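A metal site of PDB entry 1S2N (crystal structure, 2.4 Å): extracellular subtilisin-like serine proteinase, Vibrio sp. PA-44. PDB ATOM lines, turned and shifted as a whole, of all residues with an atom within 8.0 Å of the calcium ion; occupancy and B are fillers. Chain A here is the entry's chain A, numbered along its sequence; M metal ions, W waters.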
ATOM      1  N   PHE A 151      19.391  -2.655 -32.419  1.00  0.00           N
ATOM      2  CA  PHE A 151      19.258  -3.853 -33.238  1.00  0.00           C
ATOM      3  C   PHE A 151      17.920  -4.541 -33.020  1.00  0.00           C
ATOM      4  O   PHE A 151      17.658  -5.032 -31.926  1.00  0.00           O
ATOM      5  CB  PHE A 151      20.382  -4.830 -32.924  1.00  0.00           C
ATOM      6  CG  PHE A 151      21.598  -4.632 -33.759  1.00  0.00           C
ATOM      7  CD1 PHE A 151      22.346  -3.462 -33.639  1.00  0.00           C
ATOM      8  CD2 PHE A 151      21.982  -5.583 -34.673  1.00  0.00           C
ATOM      9  CE1 PHE A 151      23.472  -3.270 -34.421  1.00  0.00           C
ATOM     10  CE2 PHE A 151      23.100  -5.398 -35.458  1.00  0.00           C
ATOM     11  CZ  PHE A 151      23.849  -4.231 -35.328  1.00  0.00           C
ATOM     12  N   LEU A 153      15.770  -7.802 -33.832  1.00  0.00           N
ATOM     13  CA  LEU A 153      16.169  -9.205 -34.024  1.00  0.00           C
ATOM     14  C   LEU A 153      14.955 -10.135 -34.081  1.00  0.00           C
ATOM     15  O   LEU A 153      14.120 -10.105 -33.181  1.00  0.00           O
ATOM     16  CB  LEU A 153      17.058  -9.654 -32.861  1.00  0.00           C
ATOM     17  CG  LEU A 153      18.125  -8.701 -32.327  1.00  0.00           C
ATOM     18  CD1 LEU A 153      18.703  -9.253 -31.026  1.00  0.00           C
ATOM     19  CD2 LEU A 153      19.216  -8.482 -33.346  1.00  0.00           C
ATOM     20  N   ALA A 168      18.799 -13.701 -31.264  1.00  0.00           N
ATOM     21  CA  ALA A 168      17.545 -13.385 -30.566  1.00  0.00           C
ATOM     22  C   ALA A 168      17.669 -13.203 -29.046  1.00  0.00           C
ATOM     23  O   ALA A 168      16.998 -12.352 -28.452  1.00  0.00           O
ATOM     24  CB  ALA A 168      16.499 -14.452 -30.871  1.00  0.00           C
ATOM     25  N   ARG A 169      18.531 -14.008 -28.418  1.00  0.00           N
ATOM     26  CA  ARG A 169      18.593 -14.080 -26.951  1.00  0.00           C
ATOM     27  C   ARG A 169      19.369 -12.929 -26.308  1.00  0.00           C
ATOM     28  O   ARG A 169      19.425 -12.837 -25.085  1.00  0.00           O
ATOM     29  CB  ARG A 169      19.178 -15.425 -26.508  1.00  0.00           C
ATOM     30  CG  ARG A 169      20.675 -15.614 -26.744  1.00  0.00           C
ATOM     31  CD  ARG A 169      21.250 -16.867 -26.073  1.00  0.00           C
ATOM     32  NE  ARG A 169      22.573 -17.187 -26.607  1.00  0.00           N
ATOM     33  CZ  ARG A 169      23.346 -18.197 -26.189  1.00  0.00           C
ATOM     34  NH1 ARG A 169      22.933 -19.036 -25.239  1.00  0.00           N
ATOM     35  NH2 ARG A 169      24.535 -18.386 -26.759  1.00  0.00           N
ATOM     36  N   VAL A 170      19.968 -12.062 -27.128  1.00  0.00           N
ATOM     37  CA  VAL A 170      20.746 -10.922 -26.645  1.00  0.00           C
ATOM     38  C   VAL A 170      19.792  -9.953 -25.947  1.00  0.00           C
ATOM     39  O   VAL A 170      18.924  -9.391 -26.609  1.00  0.00           O
ATOM     40  CB  VAL A 170      21.473 -10.186 -27.810  1.00  0.00           C
ATOM     41  CG1 VAL A 170      22.209  -8.948 -27.290  1.00  0.00           C
ATOM     42  CG2 VAL A 170      22.455 -11.104 -28.521  1.00  0.00           C
ATOM     43  N   PRO A 171      19.908  -9.770 -24.627  1.00  0.00           N
ATOM     44  CA  PRO A 171      18.954  -8.931 -23.895  1.00  0.00           C
ATOM     45  C   PRO A 171      18.804  -7.503 -24.440  1.00  0.00           C
ATOM     46  O   PRO A 171      17.671  -7.063 -24.628  1.00  0.00           O
ATOM     47  CB  PRO A 171      19.523  -8.931 -22.464  1.00  0.00           C
ATOM     48  CG  PRO A 171      20.255 -10.205 -22.374  1.00  0.00           C
ATOM     49  CD  PRO A 171      20.896 -10.385 -23.728  1.00  0.00           C
ATOM     50  N   SER A 172      19.914  -6.815 -24.721  1.00  0.00           N
ATOM     51  CA  SER A 172      19.860  -5.411 -25.149  1.00  0.00           C
ATOM     52  C   SER A 172      19.219  -5.214 -26.535  1.00  0.00           C
ATOM     53  O   SER A 172      18.852  -4.109 -26.907  1.00  0.00           O
ATOM     54  CB  SER A 172      21.245  -4.770 -25.114  1.00  0.00           C
ATOM     55  OG  SER A 172      22.199  -5.579 -25.773  1.00  0.00           O
ATOM     56  N   GLY A 173      19.093  -6.296 -27.296  1.00  0.00           N
ATOM     57  CA  GLY A 173      18.355  -6.251 -28.540  1.00  0.00           C
ATOM     58  C   GLY A 173      16.849  -6.201 -28.338  1.00  0.00           C
ATOM     59  O   GLY A 173      16.327  -6.466 -27.249  1.00  0.00           O
ATOM     60  N   VAL A 174      16.145  -5.853 -29.409  1.00  0.00           N
ATOM     61  CA  VAL A 174      14.692  -5.874 -29.446  1.00  0.00           C
ATOM     62  C   VAL A 174      14.238  -7.103 -30.241  1.00  0.00           C
ATOM     63  O   VAL A 174      14.246  -7.107 -31.473  1.00  0.00           O
ATOM     64  CB  VAL A 174      14.135  -4.593 -30.085  1.00  0.00           C
ATOM     65  CG1 VAL A 174      12.616  -4.666 -30.229  1.00  0.00           C
ATOM     66  CG2 VAL A 174      14.566  -3.380 -29.266  1.00  0.00           C
ATOM     67  N   THR A 175      13.859  -8.158 -29.523  1.00  0.00           N
ATOM     68  CA  THR A 175      13.517  -9.434 -30.145  1.00  0.00           C
ATOM     69  C   THR A 175      12.018  -9.500 -30.431  1.00  0.00           C
ATOM     70  O   THR A 175      11.203  -9.277 -29.553  1.00  0.00           O
ATOM     71  CB  THR A 175      13.987 -10.570 -29.226  1.00  0.00           C
ATOM     72  OG1 THR A 175      15.408 -10.465 -29.029  1.00  0.00           O
ATOM     73  CG2 THR A 175      13.805 -11.949 -29.874  1.00  0.00           C
ATOM     74  N   VAL A 176      11.670  -9.807 -31.674  1.00  0.00           N
ATOM     75  CA  VAL A 176      10.302  -9.622 -32.175  1.00  0.00           C
ATOM     76  C   VAL A 176       9.661 -10.947 -32.566  1.00  0.00           C
ATOM     77  O   VAL A 176      10.175 -11.680 -33.400  1.00  0.00           O
ATOM     78  CB  VAL A 176      10.299  -8.675 -33.394  1.00  0.00           C
ATOM     79  CG1 VAL A 176       8.880  -8.283 -33.782  1.00  0.00           C
ATOM     80  CG2 VAL A 176      11.136  -7.428 -33.104  1.00  0.00           C
ATOM     81  N   SER A 193      10.569 -15.334 -22.462  1.00  0.00           N
ATOM     82  CA  SER A 193      11.059 -14.175 -21.727  1.00  0.00           C
ATOM     83  C   SER A 193      12.061 -13.331 -22.527  1.00  0.00           C
ATOM     84  O   SER A 193      12.344 -12.191 -22.143  1.00  0.00           O
ATOM     85  CB  SER A 193      11.691 -14.622 -20.420  1.00  0.00           C
ATOM     86  OG  SER A 193      12.769 -15.501 -20.668  1.00  0.00           O
ATOM     87  N   CYS A 194      12.604 -13.873 -23.614  1.00  0.00           N
ATOM     88  CA  CYS A 194      13.561 -13.135 -24.440  1.00  0.00           C
ATOM     89  C   CYS A 194      12.889 -12.271 -25.495  1.00  0.00           C
ATOM     90  O   CYS A 194      13.510 -11.373 -26.050  1.00  0.00           O
ATOM     91  CB  CYS A 194      14.547 -14.085 -25.120  1.00  0.00           C
ATOM     92  SG  CYS A 194      15.747 -14.741 -23.983  1.00  0.00           S
ATOM     93  N   VAL A 195      11.613 -12.546 -25.763  1.00  0.00           N
ATOM     94  CA  VAL A 195      10.868 -11.753 -26.720  1.00  0.00           C
ATOM     95  C   VAL A 195      10.347 -10.480 -26.054  1.00  0.00           C
ATOM     96  O   VAL A 195       9.665 -10.530 -25.039  1.00  0.00           O
ATOM     97  CB  VAL A 195       9.708 -12.548 -27.350  1.00  0.00           C
ATOM     98  CG1 VAL A 195       8.948 -11.698 -28.375  1.00  0.00           C
ATOM     99  CG2 VAL A 195      10.250 -13.833 -27.997  1.00  0.00           C
ATOM    100  N   ASP A 196      10.709  -9.340 -26.620  1.00  0.00           N
ATOM    101  CA  ASP A 196      10.295  -8.034 -26.113  1.00  0.00           C
ATOM    102  C   ASP A 196       8.904  -7.628 -26.568  1.00  0.00           C
ATOM    103  O   ASP A 196       8.162  -7.031 -25.787  1.00  0.00           O
ATOM    104  CB  ASP A 196      11.296  -6.955 -26.524  1.00  0.00           C
ATOM    105  CG  ASP A 196      12.680  -7.184 -25.951  1.00  0.00           C
ATOM    106  OD1 ASP A 196      12.920  -6.801 -24.778  1.00  0.00           O
ATOM    107  OD2 ASP A 196      13.591  -7.760 -26.583  1.00  0.00           O
ATOM    108  N   LEU A 197       8.563  -7.909 -27.823  1.00  0.00           N
ATOM    109  CA  LEU A 197       7.229  -7.563 -28.334  1.00  0.00           C
ATOM    110  C   LEU A 197       6.834  -8.326 -29.598  1.00  0.00           C
ATOM    111  O   LEU A 197       7.653  -8.992 -30.215  1.00  0.00           O
ATOM    112  CB  LEU A 197       7.105  -6.050 -28.576  1.00  0.00           C
ATOM    113  CG  LEU A 197       7.587  -5.448 -29.900  1.00  0.00           C
ATOM    114  CD1 LEU A 197       7.087  -4.023 -30.057  1.00  0.00           C
ATOM    115  CD2 LEU A 197       9.094  -5.496 -29.964  1.00  0.00           C
ATOM    116  N   THR A 246      14.250   1.252 -26.897  1.00  0.00           N
ATOM    117  CA  THR A 246      13.672   0.013 -26.361  1.00  0.00           C
ATOM    118  C   THR A 246      12.547   0.342 -25.394  1.00  0.00           C
ATOM    119  O   THR A 246      11.501  -0.290 -25.406  1.00  0.00           O
ATOM    120  CB  THR A 246      14.760  -0.814 -25.645  1.00  0.00           C
ATOM    121  OG1 THR A 246      15.674  -1.366 -26.596  1.00  0.00           O
ATOM    122  CG2 THR A 246      14.171  -2.042 -24.928  1.00  0.00           C
ATOM    123  N   ASN A 250       8.374  -0.118 -25.874  1.00  0.00           N
ATOM    124  CA  ASN A 250       7.695  -0.881 -24.830  1.00  0.00           C
ATOM    125  C   ASN A 250       6.481  -0.148 -24.250  1.00  0.00           C
ATOM    126  O   ASN A 250       5.421  -0.746 -24.062  1.00  0.00           O
ATOM    127  CB  ASN A 250       8.662  -1.224 -23.690  1.00  0.00           C
ATOM    128  CG  ASN A 250       9.315  -2.573 -23.873  1.00  0.00           C
ATOM    129  OD1 ASN A 250      10.461  -2.657 -24.308  1.00  0.00           O
ATOM    130  ND2 ASN A 250       8.598  -3.634 -23.546  1.00  0.00           N
HETATM  131 CA    CA M   1      15.423  -7.404 -25.123  1.00  0.00          CA
HETATM  132  O   HOH W   1      15.108  -7.805 -22.648  1.00  0.00           O
HETATM  133  O   HOH W   2      16.320  -9.424 -26.430  1.00  0.00           O
HETATM  134  O   HOH W   3      14.261  -9.415 -24.357  1.00  0.00           O
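N of Asp 196 is in hydrogen-bond range of O of Thr 175 (3.0 Å).
Within 4 Å of the calcium ion: Pro 171, Gly 173 and Asp 196. The nearest printed residue that does not touch the calcium ion is Val 170 (4.3 Å).
The calcium ion is bound by O of Pro 171 (2.3 Å), OD2 of Asp 196 (2.4 Å), water W3 (2.4 Å), O of Gly 173 (2.5 Å), water W1 (2.5 Å), water W2 (2.6 Å) and OD1 of Asp 196 (2.6 Å).
Water W2 lies within hydrogen-bond range of the backbone carbonyl oxygen (O) of Val 170 (2.6 Å), the side-chain hydroxyl (OG1) of Thr 175 (2.9 Å) and the backbone carbonyl oxygen (O) of Cys 194 (3.4 Å).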
